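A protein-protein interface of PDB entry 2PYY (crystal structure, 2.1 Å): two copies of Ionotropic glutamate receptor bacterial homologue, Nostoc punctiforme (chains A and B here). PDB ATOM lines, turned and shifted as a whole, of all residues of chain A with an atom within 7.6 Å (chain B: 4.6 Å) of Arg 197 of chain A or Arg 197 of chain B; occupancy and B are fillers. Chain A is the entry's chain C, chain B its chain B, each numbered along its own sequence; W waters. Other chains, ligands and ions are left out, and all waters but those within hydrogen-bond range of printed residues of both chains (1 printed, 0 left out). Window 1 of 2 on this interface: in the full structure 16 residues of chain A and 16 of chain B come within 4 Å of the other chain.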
ATOM      1  N   ILE A  38     -12.517   3.184  -7.109  1.00  0.00           N
ATOM      2  CA  ILE A  38     -11.130   2.850  -7.383  1.00  0.00           C
ATOM      3  C   ILE A  38     -11.032   1.580  -8.216  1.00  0.00           C
ATOM      4  O   ILE A  38     -10.150   1.446  -9.065  1.00  0.00           O
ATOM      5  CB  ILE A  38     -10.374   2.633  -6.063  1.00  0.00           C
ATOM      6  CG1 ILE A  38     -10.370   3.932  -5.253  1.00  0.00           C
ATOM      7  CG2 ILE A  38      -8.969   2.147  -6.337  1.00  0.00           C
ATOM      8  CD1 ILE A  38      -9.783   3.788  -3.864  1.00  0.00           C
ATOM      9  N   GLU A  76      -2.036  12.463  13.519  1.00  0.00           N
ATOM     10  CA  GLU A  76      -1.429  12.844  12.250  1.00  0.00           C
ATOM     11  C   GLU A  76       0.090  12.792  12.378  1.00  0.00           C
ATOM     12  O   GLU A  76       0.808  12.607  11.394  1.00  0.00           O
ATOM     13  CB  GLU A  76      -1.895  14.253  11.862  1.00  0.00           C
ATOM     14  CG  GLU A  76      -1.530  14.691  10.449  1.00  0.00           C
ATOM     15  CD  GLU A  76      -0.071  15.056  10.319  1.00  0.00           C
ATOM     16  OE1 GLU A  76       0.398  15.917  11.104  1.00  0.00           O
ATOM     17  OE2 GLU A  76       0.606  14.492   9.430  1.00  0.00           O
ATOM     18  N   PHE A  79       0.577   8.925  12.010  1.00  0.00           N
ATOM     19  CA  PHE A  79      -0.142   8.306  10.899  1.00  0.00           C
ATOM     20  C   PHE A  79      -0.567   9.353   9.869  1.00  0.00           C
ATOM     21  O   PHE A  79      -0.260  10.537  10.011  1.00  0.00           O
ATOM     22  CB  PHE A  79      -1.372   7.549  11.416  1.00  0.00           C
ATOM     23  CG  PHE A  79      -1.050   6.526  12.477  1.00  0.00           C
ATOM     24  CD1 PHE A  79      -0.947   6.900  13.811  1.00  0.00           C
ATOM     25  CD2 PHE A  79      -0.799   5.200  12.131  1.00  0.00           C
ATOM     26  CE1 PHE A  79      -0.594   5.973  14.790  1.00  0.00           C
ATOM     27  CE2 PHE A  79      -0.445   4.264  13.104  1.00  0.00           C
ATOM     28  CZ  PHE A  79      -0.342   4.654  14.432  1.00  0.00           C
ATOM     29  N   ASP A  80      -1.277   8.907   8.837  1.00  0.00           N
ATOM     30  CA  ASP A  80      -1.740   9.796   7.775  1.00  0.00           C
ATOM     31  C   ASP A  80      -3.264   9.723   7.675  1.00  0.00           C
ATOM     32  O   ASP A  80      -3.894   8.820   8.223  1.00  0.00           O
ATOM     33  CB  ASP A  80      -1.118   9.374   6.433  1.00  0.00           C
ATOM     34  CG  ASP A  80      -0.798  10.552   5.523  1.00  0.00           C
ATOM     35  OD1 ASP A  80      -1.459  11.615   5.642  1.00  0.00           O
ATOM     36  OD2 ASP A  80       0.112  10.401   4.672  1.00  0.00           O
ATOM     37  N   PHE A  81      -3.848  10.684   6.970  1.00  0.00           N
ATOM     38  CA  PHE A  81      -5.291  10.723   6.793  1.00  0.00           C
ATOM     39  C   PHE A  81      -5.652  11.160   5.395  1.00  0.00           C
ATOM     40  O   PHE A  81      -4.884  11.837   4.722  1.00  0.00           O
ATOM     41  CB  PHE A  81      -5.949  11.706   7.758  1.00  0.00           C
ATOM     42  CG  PHE A  81      -6.016  11.233   9.173  1.00  0.00           C
ATOM     43  CD1 PHE A  81      -4.953  11.432  10.042  1.00  0.00           C
ATOM     44  CD2 PHE A  81      -7.171  10.622   9.650  1.00  0.00           C
ATOM     45  CE1 PHE A  81      -5.046  11.030  11.376  1.00  0.00           C
ATOM     46  CE2 PHE A  81      -7.270  10.222  10.971  1.00  0.00           C
ATOM     47  CZ  PHE A  81      -6.209  10.427  11.837  1.00  0.00           C
ATOM     48  N   SER A  82      -6.838  10.759   4.964  1.00  0.00           N
ATOM     49  CA  SER A  82      -7.339  11.145   3.660  1.00  0.00           C
ATOM     50  C   SER A  82      -8.034  12.476   3.922  1.00  0.00           C
ATOM     51  O   SER A  82      -8.045  12.974   5.054  1.00  0.00           O
ATOM     52  CB  SER A  82      -8.393  10.150   3.191  1.00  0.00           C
ATOM     53  OG  SER A  82      -9.532  10.208   4.044  1.00  0.00           O
ATOM     54  N   LEU A  83      -8.625  13.037   2.877  1.00  0.00           N
ATOM     55  CA  LEU A  83      -9.373  14.269   3.007  1.00  0.00           C
ATOM     56  C   LEU A  83     -10.494  13.943   3.991  1.00  0.00           C
ATOM     57  O   LEU A  83     -10.922  12.803   4.098  1.00  0.00           O
ATOM     58  CB  LEU A  83      -9.984  14.649   1.660  1.00  0.00           C
ATOM     59  CG  LEU A  83      -9.079  15.359   0.669  1.00  0.00           C
ATOM     60  CD1 LEU A  83      -9.689  15.317  -0.734  1.00  0.00           C
ATOM     61  CD2 LEU A  83      -8.895  16.813   1.126  1.00  0.00           C
ATOM     62  N   ILE A 188     -10.300   9.036   6.885  1.00  0.00           N
ATOM     63  CA  ILE A 188      -9.946   7.642   6.718  1.00  0.00           C
ATOM     64  C   ILE A 188      -8.478   7.609   7.115  1.00  0.00           C
ATOM     65  O   ILE A 188      -7.642   8.288   6.510  1.00  0.00           O
ATOM     66  CB  ILE A 188     -10.135   7.189   5.250  1.00  0.00           C
ATOM     67  CG1 ILE A 188     -11.619   7.269   4.887  1.00  0.00           C
ATOM     68  CG2 ILE A 188      -9.621   5.768   5.061  1.00  0.00           C
ATOM     69  CD1 ILE A 188     -11.953   6.889   3.434  1.00  0.00           C
ATOM     70  N   LEU A 190      -4.730   6.093   7.647  1.00  0.00           N
ATOM     71  CA  LEU A 190      -3.838   5.191   6.936  1.00  0.00           C
ATOM     72  C   LEU A 190      -2.405   5.254   7.453  1.00  0.00           C
ATOM     73  O   LEU A 190      -2.042   6.136   8.235  1.00  0.00           O
ATOM     74  CB  LEU A 190      -3.826   5.523   5.437  1.00  0.00           C
ATOM     75  CG  LEU A 190      -5.134   5.485   4.651  1.00  0.00           C
ATOM     76  CD1 LEU A 190      -5.765   6.877   4.660  1.00  0.00           C
ATOM     77  CD2 LEU A 190      -4.860   5.052   3.228  1.00  0.00           C
ATOM     78  N   PRO A 191      -1.572   4.287   7.045  1.00  0.00           N
ATOM     79  CA  PRO A 191      -0.191   4.340   7.513  1.00  0.00           C
ATOM     80  C   PRO A 191       0.501   5.393   6.649  1.00  0.00           C
ATOM     81  O   PRO A 191      -0.027   5.795   5.606  1.00  0.00           O
ATOM     82  CB  PRO A 191       0.320   2.926   7.245  1.00  0.00           C
ATOM     83  CG  PRO A 191      -0.486   2.499   6.050  1.00  0.00           C
ATOM     84  CD  PRO A 191      -1.861   3.011   6.372  1.00  0.00           C
ATOM     85  N   ASN A 192       1.663   5.854   7.087  1.00  0.00           N
ATOM     86  CA  ASN A 192       2.388   6.836   6.313  1.00  0.00           C
ATOM     87  C   ASN A 192       2.823   6.230   4.989  1.00  0.00           C
ATOM     88  O   ASN A 192       2.942   5.013   4.864  1.00  0.00           O
ATOM     89  CB  ASN A 192       3.607   7.349   7.081  1.00  0.00           C
ATOM     90  CG  ASN A 192       3.237   8.393   8.107  1.00  0.00           C
ATOM     91  OD1 ASN A 192       2.291   9.163   7.910  1.00  0.00           O
ATOM     92  ND2 ASN A 192       3.977   8.432   9.209  1.00  0.00           N
ATOM     93  N   ASN A 193       3.026   7.093   4.000  1.00  0.00           N
ATOM     94  CA  ASN A 193       3.451   6.684   2.669  1.00  0.00           C
ATOM     95  C   ASN A 193       2.556   5.648   2.021  1.00  0.00           C
ATOM     96  O   ASN A 193       3.002   4.866   1.176  1.00  0.00           O
ATOM     97  CB  ASN A 193       4.882   6.174   2.722  1.00  0.00           C
ATOM     98  CG  ASN A 193       5.824   7.189   3.342  1.00  0.00           C
ATOM     99  OD1 ASN A 193       5.976   7.245   4.565  1.00  0.00           O
ATOM    100  ND2 ASN A 193       6.438   8.018   2.504  1.00  0.00           N
ATOM    101  N   SER A 194       1.292   5.629   2.423  1.00  0.00           N
ATOM    102  CA  SER A 194       0.358   4.682   1.838  1.00  0.00           C
ATOM    103  C   SER A 194       0.092   5.019   0.383  1.00  0.00           C
ATOM    104  O   SER A 194      -0.200   6.163   0.042  1.00  0.00           O
ATOM    105  CB  SER A 194      -0.977   4.687   2.573  1.00  0.00           C
ATOM    106  OG  SER A 194      -1.968   4.080   1.751  1.00  0.00           O
ATOM    107  N   PRO A 195       0.168   4.013  -0.496  1.00  0.00           N
ATOM    108  CA  PRO A 195      -0.071   4.210  -1.925  1.00  0.00           C
ATOM    109  C   PRO A 195      -1.554   4.350  -2.257  1.00  0.00           C
ATOM    110  O   PRO A 195      -1.915   4.616  -3.396  1.00  0.00           O
ATOM    111  CB  PRO A 195       0.548   2.965  -2.544  1.00  0.00           C
ATOM    112  CG  PRO A 195       0.280   1.916  -1.503  1.00  0.00           C
ATOM    113  CD  PRO A 195       0.632   2.641  -0.221  1.00  0.00           C
ATOM    114  N   TYR A 196      -2.413   4.173  -1.261  1.00  0.00           N
ATOM    115  CA  TYR A 196      -3.843   4.287  -1.500  1.00  0.00           C
ATOM    116  C   TYR A 196      -4.446   5.631  -1.076  1.00  0.00           C
ATOM    117  O   TYR A 196      -5.617   5.901  -1.350  1.00  0.00           O
ATOM    118  CB  TYR A 196      -4.583   3.151  -0.790  1.00  0.00           C
ATOM    119  CG  TYR A 196      -4.080   1.770  -1.158  1.00  0.00           C
ATOM    120  CD1 TYR A 196      -3.196   1.085  -0.326  1.00  0.00           C
ATOM    121  CD2 TYR A 196      -4.467   1.161  -2.356  1.00  0.00           C
ATOM    122  CE1 TYR A 196      -2.710  -0.173  -0.674  1.00  0.00           C
ATOM    123  CE2 TYR A 196      -3.982  -0.098  -2.714  1.00  0.00           C
ATOM    124  CZ  TYR A 196      -3.104  -0.758  -1.870  1.00  0.00           C
ATOM    125  OH  TYR A 196      -2.614  -1.995  -2.217  1.00  0.00           O
ATOM    126  N   ARG A 197      -3.663   6.474  -0.408  1.00  0.00           N
ATOM    127  CA  ARG A 197      -4.188   7.763   0.034  1.00  0.00           C
ATOM    128  C   ARG A 197      -4.731   8.583  -1.143  1.00  0.00           C
ATOM    129  O   ARG A 197      -5.884   8.994  -1.123  1.00  0.00           O
ATOM    130  CB  ARG A 197      -3.110   8.563   0.783  1.00  0.00           C
ATOM    131  CG  ARG A 197      -3.612   9.886   1.387  1.00  0.00           C
ATOM    132  CD  ARG A 197      -2.508  10.633   2.149  1.00  0.00           C
ATOM    133  NE  ARG A 197      -1.378  11.001   1.287  1.00  0.00           N
ATOM    134  CZ  ARG A 197      -1.375  12.033   0.448  1.00  0.00           C
ATOM    135  NH1 ARG A 197      -2.442  12.817   0.349  1.00  0.00           N
ATOM    136  NH2 ARG A 197      -0.306  12.281  -0.300  1.00  0.00           N
ATOM    137  N   LYS A 198      -3.919   8.802  -2.176  1.00  0.00           N
ATOM    138  CA  LYS A 198      -4.373   9.594  -3.316  1.00  0.00           C
ATOM    139  C   LYS A 198      -5.581   9.004  -4.046  1.00  0.00           C
ATOM    140  O   LYS A 198      -6.552   9.717  -4.334  1.00  0.00           O
ATOM    141  CB  LYS A 198      -3.222   9.837  -4.294  1.00  0.00           C
ATOM    142  CG  LYS A 198      -2.082  10.635  -3.671  1.00  0.00           C
ATOM    143  CD  LYS A 198      -1.138  11.218  -4.726  1.00  0.00           C
ATOM    144  CE  LYS A 198      -1.783  12.397  -5.451  1.00  0.00           C
ATOM    145  NZ  LYS A 198      -2.052  13.524  -4.524  1.00  0.00           N
ATOM    146  N   PRO A 199      -5.549   7.698  -4.363  1.00  0.00           N
ATOM    147  CA  PRO A 199      -6.717   7.139  -5.057  1.00  0.00           C
ATOM    148  C   PRO A 199      -7.959   7.211  -4.171  1.00  0.00           C
ATOM    149  O   PRO A 199      -9.084   7.312  -4.666  1.00  0.00           O
ATOM    150  CB  PRO A 199      -6.284   5.708  -5.395  1.00  0.00           C
ATOM    151  CG  PRO A 199      -5.255   5.396  -4.378  1.00  0.00           C
ATOM    152  CD  PRO A 199      -4.482   6.695  -4.224  1.00  0.00           C
ATOM    153  N   ILE A 200      -7.754   7.165  -2.854  1.00  0.00           N
ATOM    154  CA  ILE A 200      -8.887   7.287  -1.945  1.00  0.00           C
ATOM    155  C   ILE A 200      -9.428   8.724  -2.014  1.00  0.00           C
ATOM    156  O   ILE A 200     -10.627   8.939  -2.198  1.00  0.00           O
ATOM    157  CB  ILE A 200      -8.496   6.925  -0.480  1.00  0.00           C
ATOM    158  CG1 ILE A 200      -8.389   5.402  -0.338  1.00  0.00           C
ATOM    159  CG2 ILE A 200      -9.549   7.449   0.498  1.00  0.00           C
ATOM    160  CD1 ILE A 200      -7.924   4.931   1.028  1.00  0.00           C
ATOM    161  N   ASN A 201      -8.540   9.706  -1.902  1.00  0.00           N
ATOM    162  CA  ASN A 201      -8.959  11.106  -1.967  1.00  0.00           C
ATOM    163  C   ASN A 201      -9.628  11.397  -3.308  1.00  0.00           C
ATOM    164  O   ASN A 201     -10.669  12.047  -3.375  1.00  0.00           O
ATOM    165  CB  ASN A 201      -7.748  12.029  -1.783  1.00  0.00           C
ATOM    166  CG  ASN A 201      -7.204  11.989  -0.374  1.00  0.00           C
ATOM    167  OD1 ASN A 201      -7.906  11.586   0.547  1.00  0.00           O
ATOM    168  ND2 ASN A 201      -5.950  12.414  -0.195  1.00  0.00           N
ATOM    169  N   GLN A 202      -8.990  10.917  -4.367  1.00  0.00           N
ATOM    170  CA  GLN A 202      -9.471  11.066  -5.735  1.00  0.00           C
ATOM    171  C   GLN A 202     -10.913  10.555  -5.849  1.00  0.00           C
ATOM    172  O   GLN A 202     -11.785  11.257  -6.345  1.00  0.00           O
ATOM    173  CB  GLN A 202      -8.554  10.264  -6.661  1.00  0.00           C
ATOM    174  CG  GLN A 202      -8.897  10.316  -8.128  1.00  0.00           C
ATOM    175  CD  GLN A 202      -8.756  11.702  -8.706  1.00  0.00           C
ATOM    176  OE1 GLN A 202      -7.885  12.469  -8.291  1.00  0.00           O
ATOM    177  NE2 GLN A 202      -9.603  12.029  -9.679  1.00  0.00           N
ATOM    178  N   ALA A 203     -11.156   9.334  -5.374  1.00  0.00           N
ATOM    179  CA  ALA A 203     -12.487   8.726  -5.424  1.00  0.00           C
ATOM    180  C   ALA A 203     -13.494   9.539  -4.622  1.00  0.00           C
ATOM    181  O   ALA A 203     -14.610   9.817  -5.069  1.00  0.00           O
ATOM    182  CB  ALA A 203     -12.431   7.305  -4.877  1.00  0.00           C
ATOM    183  N   LEU A 204     -13.086   9.901  -3.416  1.00  0.00           N
ATOM    184  CA  LEU A 204     -13.931  10.677  -2.532  1.00  0.00           C
ATOM    185  C   LEU A 204     -14.316  11.983  -3.217  1.00  0.00           C
ATOM    186  O   LEU A 204     -15.480  12.381  -3.197  1.00  0.00           O
ATOM    187  CB  LEU A 204     -13.184  10.963  -1.234  1.00  0.00           C
ATOM    188  CG  LEU A 204     -13.953  11.730  -0.165  1.00  0.00           C
ATOM    189  CD1 LEU A 204     -15.150  10.911   0.310  1.00  0.00           C
ATOM    190  CD2 LEU A 204     -13.013  12.025   0.992  1.00  0.00           C
ATOM    191  N   ASP B  80      -0.872  17.512  -4.797  1.00  0.00           N
ATOM    192  CA  ASP B  80      -1.237  17.118  -3.445  1.00  0.00           C
ATOM    193  C   ASP B  80      -1.878  18.307  -2.719  1.00  0.00           C
ATOM    194  O   ASP B  80      -1.625  19.463  -3.060  1.00  0.00           O
ATOM    195  CB  ASP B  80       0.004  16.652  -2.681  1.00  0.00           C
ATOM    196  CG  ASP B  80      -0.172  15.277  -2.062  1.00  0.00           C
ATOM    197  OD1 ASP B  80      -1.334  14.847  -1.905  1.00  0.00           O
ATOM    198  OD2 ASP B  80       0.846  14.641  -1.712  1.00  0.00           O
ATOM    199  N   PHE B  81      -2.704  18.010  -1.723  1.00  0.00           N
ATOM    200  CA  PHE B  81      -3.370  19.037  -0.945  1.00  0.00           C
ATOM    201  C   PHE B  81      -3.221  18.775   0.548  1.00  0.00           C
ATOM    202  O   PHE B  81      -3.120  17.629   0.975  1.00  0.00           O
ATOM    203  CB  PHE B  81      -4.867  19.084  -1.268  1.00  0.00           C
ATOM    204  CG  PHE B  81      -5.209  19.871  -2.499  1.00  0.00           C
ATOM    205  CD1 PHE B  81      -5.465  19.228  -3.701  1.00  0.00           C
ATOM    206  CD2 PHE B  81      -5.270  21.257  -2.457  1.00  0.00           C
ATOM    207  CE1 PHE B  81      -5.779  19.956  -4.852  1.00  0.00           C
ATOM    208  CE2 PHE B  81      -5.582  21.997  -3.599  1.00  0.00           C
ATOM    209  CZ  PHE B  81      -5.834  21.343  -4.797  1.00  0.00           C
ATOM    210  N   LEU B 190       0.169  21.537  -3.093  1.00  0.00           N
ATOM    211  CA  LEU B 190       1.575  21.179  -3.009  1.00  0.00           C
ATOM    212  C   LEU B 190       1.928  20.196  -4.104  1.00  0.00           C
ATOM    213  O   LEU B 190       1.045  19.553  -4.671  1.00  0.00           O
ATOM    214  CB  LEU B 190       1.833  20.484  -1.668  1.00  0.00           C
ATOM    215  CG  LEU B 190       1.290  21.156  -0.420  1.00  0.00           C
ATOM    216  CD1 LEU B 190       0.646  20.133   0.502  1.00  0.00           C
ATOM    217  CD2 LEU B 190       2.413  21.890   0.260  1.00  0.00           C
ATOM    218  N   SER B 194       5.462  16.028  -1.516  1.00  0.00           N
ATOM    219  CA  SER B 194       6.041  17.171  -0.835  1.00  0.00           C
ATOM    220  C   SER B 194       6.258  16.855   0.634  1.00  0.00           C
ATOM    221  O   SER B 194       5.357  16.366   1.318  1.00  0.00           O
ATOM    222  CB  SER B 194       5.131  18.390  -0.955  1.00  0.00           C
ATOM    223  OG  SER B 194       5.512  19.383  -0.019  1.00  0.00           O
ATOM    224  N   PRO B 195       7.470  17.111   1.135  1.00  0.00           N
ATOM    225  CA  PRO B 195       7.791  16.853   2.540  1.00  0.00           C
ATOM    226  C   PRO B 195       7.173  17.881   3.484  1.00  0.00           C
ATOM    227  O   PRO B 195       7.292  17.750   4.694  1.00  0.00           O
ATOM    228  CB  PRO B 195       9.315  16.899   2.553  1.00  0.00           C
ATOM    229  CG  PRO B 195       9.612  17.919   1.490  1.00  0.00           C
ATOM    230  CD  PRO B 195       8.679  17.489   0.382  1.00  0.00           C
ATOM    231  N   TYR B 196       6.514  18.900   2.933  1.00  0.00           N
ATOM    232  CA  TYR B 196       5.892  19.930   3.764  1.00  0.00           C
ATOM    233  C   TYR B 196       4.420  19.655   4.072  1.00  0.00           C
ATOM    234  O   TYR B 196       3.827  20.294   4.947  1.00  0.00           O
ATOM    235  CB  TYR B 196       6.036  21.303   3.099  1.00  0.00           C
ATOM    236  CG  TYR B 196       7.485  21.734   2.953  1.00  0.00           C
ATOM    237  CD1 TYR B 196       8.098  21.794   1.697  1.00  0.00           C
ATOM    238  CD2 TYR B 196       8.261  22.023   4.082  1.00  0.00           C
ATOM    239  CE1 TYR B 196       9.453  22.128   1.571  1.00  0.00           C
ATOM    240  CE2 TYR B 196       9.612  22.356   3.968  1.00  0.00           C
ATOM    241  CZ  TYR B 196      10.201  22.405   2.717  1.00  0.00           C
ATOM    242  OH  TYR B 196      11.539  22.707   2.621  1.00  0.00           O
ATOM    243  N   ARG B 197       3.835  18.693   3.366  1.00  0.00           N
ATOM    244  CA  ARG B 197       2.432  18.358   3.568  1.00  0.00           C
ATOM    245  C   ARG B 197       2.081  18.029   5.018  1.00  0.00           C
ATOM    246  O   ARG B 197       1.281  18.728   5.640  1.00  0.00           O
ATOM    247  CB  ARG B 197       2.017  17.181   2.679  1.00  0.00           C
ATOM    248  CG  ARG B 197       0.530  16.847   2.787  1.00  0.00           C
ATOM    249  CD  ARG B 197       0.135  15.748   1.809  1.00  0.00           C
ATOM    250  NE  ARG B 197       0.804  14.491   2.134  1.00  0.00           N
ATOM    251  CZ  ARG B 197       0.332  13.598   2.993  1.00  0.00           C
ATOM    252  NH1 ARG B 197      -0.827  13.812   3.608  1.00  0.00           N
ATOM    253  NH2 ARG B 197       1.032  12.504   3.256  1.00  0.00           N
ATOM    254  N   LYS B 198       2.684  16.975   5.560  1.00  0.00           N
ATOM    255  CA  LYS B 198       2.399  16.571   6.938  1.00  0.00           C
ATOM    256  C   LYS B 198       2.664  17.659   7.991  1.00  0.00           C
ATOM    257  O   LYS B 198       1.839  17.888   8.870  1.00  0.00           O
ATOM    258  CB  LYS B 198       3.146  15.267   7.271  1.00  0.00           C
ATOM    259  CG  LYS B 198       2.672  14.080   6.422  1.00  0.00           C
ATOM    260  CD  LYS B 198       3.413  12.774   6.743  1.00  0.00           C
ATOM    261  CE  LYS B 198       3.255  12.387   8.221  1.00  0.00           C
ATOM    262  NZ  LYS B 198       1.807  12.314   8.611  1.00  0.00           N
ATOM    263  N   PRO B 199       3.808  18.353   7.920  1.00  0.00           N
ATOM    264  CA  PRO B 199       4.027  19.391   8.933  1.00  0.00           C
ATOM    265  C   PRO B 199       3.003  20.527   8.827  1.00  0.00           C
ATOM    266  O   PRO B 199       2.676  21.178   9.822  1.00  0.00           O
ATOM    267  CB  PRO B 199       5.460  19.857   8.658  1.00  0.00           C
ATOM    268  CG  PRO B 199       5.625  19.602   7.216  1.00  0.00           C
ATOM    269  CD  PRO B 199       4.977  18.238   7.038  1.00  0.00           C
ATOM    270  N   ILE B 200       2.498  20.768   7.622  1.00  0.00           N
ATOM    271  CA  ILE B 200       1.500  21.810   7.445  1.00  0.00           C
ATOM    272  C   ILE B 200       0.208  21.328   8.086  1.00  0.00           C
ATOM    273  O   ILE B 200      -0.452  22.076   8.800  1.00  0.00           O
ATOM    274  CB  ILE B 200       1.259  22.122   5.931  1.00  0.00           C
ATOM    275  CG1 ILE B 200       2.420  22.946   5.386  1.00  0.00           C
ATOM    276  CG2 ILE B 200      -0.046  22.893   5.743  1.00  0.00           C
ATOM    277  CD1 ILE B 200       2.277  23.332   3.916  1.00  0.00           C
ATOM    278  N   ASN B 201      -0.143  20.071   7.847  1.00  0.00           N
ATOM    279  CA  ASN B 201      -1.363  19.523   8.427  1.00  0.00           C
ATOM    280  C   ASN B 201      -1.262  19.572   9.940  1.00  0.00           C
ATOM    281  O   ASN B 201      -2.197  19.980  10.622  1.00  0.00           O
ATOM    282  CB  ASN B 201      -1.569  18.082   7.960  1.00  0.00           C
ATOM    283  CG  ASN B 201      -1.982  18.002   6.515  1.00  0.00           C
ATOM    284  OD1 ASN B 201      -2.293  19.011   5.894  1.00  0.00           O
ATOM    285  ND2 ASN B 201      -2.012  16.791   5.973  1.00  0.00           N
HETATM  286  O   HOH W   1       2.752   9.889   4.454  1.00  0.00           O
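The guanidinium group (NH2) of Arg 197 of chain A is in salt-bridge range of the side-chain carboxylate (OD2) of Asp 80 of chain B, at 3.0 Å. The side-chain carboxylate (OD1) of Asp 80 of chain B is in salt-bridge range of the side-chain amino group (NZ) of Lys 198 of chain A, 3.0 Å away. NH2 of Arg 197 of chain B lies within salt-bridge range of OD2 of Asp 80 of chain A (2.7 Å). OE2 of Glu 76 of chain A is in salt-bridge range of NZ of Lys 198 of chain B (2.6 Å). The side-chain amino group (NZ) of Lys 198 of chain B is in hydrogen-bond range of the backbone carbonyl oxygen (O) of Phe 79 of chain A (3.1 Å). NZ of Lys 198 of chain B sits at hydrogen-bond distance from OD1 of Asn 192 of chain A (3.3 Å). The guanidinium group of Arg 197 of chain A sits close to the guanidinium group of Arg 197 of chain B (3.5 Å).
O of Asp 80 of chain B lies within hydrogen-bond range of N of Leu 190 of chain B (2.7 Å). OD2 of Asp 80 of chain B lies within salt-bridge range of NE of Arg 197 of chain B (3.8 Å). O of Asp 80 of chain A is in hydrogen-bond range of N of Leu 190 of chain A. The guanidinium group of Arg 197 of chain A is in salt-bridge range of the side-chain carboxylate of Asp 80 of chain A, 3.7 Å away.
Of the printed residues of chain B, Asp 80 of chain A touches Arg 197. Of the printed residues of chain B, Asn 192 of chain A touches Lys 198. Arg 197 of chain A touches two residues of chain B. Of the printed residues of chain B, Lys 198 of chain A touches Asp 80 (3.0 Å). Leu 204 of chain A touches none of the printed residues of chain B. Pro 199 of chain B touches none of the printed residues of chain A. The nearest printed residue of chain B that does not touch Arg 197 of chain A is Phe 81 of chain B (4.9 Å). The nearest residue of chain A that does not touch Arg 197 of chain B is Phe 81 of chain A (4.6 Å).
Printed residues of chain B that touch a printed residue of chain A: Asp 80, Arg 197 and Lys 198. Among the printed residues, Asp or Glu carboxylates within 4 Å of a Lys or Arg side-chain nitrogen of the other chain: Glu 76 of chain A with Lys 198 of chain B (2.6 Å), Asp 80 of chain A with Arg 197 of chain B (2.7 Å), Arg 197 of chain A with Asp 80 of chain B (3.0 Å) and Lys 198 of chain A with Asp 80 of chain B (3.0 Å).
Asp 80 of chain A touches Arg 197 of chain B, and with the chains exchanged Arg 197 of chain A touches Asp 80 of chain B. Arg 197 of chain A touches its own counterpart, Arg 197 of chain B. Lys 198 of chain A touches Asp 80 of chain B, but with the chains exchanged Asp 80 of chain A does not touch Lys 198 of chain B (4.4 Å). Of the 7 pairs that touch across the chains among the printed residues, 3 have their exchanged pair printed and touching as well.
Water W1 lies within hydrogen-bond range of OD2 of Asp 80 of chain A (2.7 Å), N of Asn 193 of chain A (2.8 Å) and NH2 of Arg 197 of chain B (3.4 Å).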
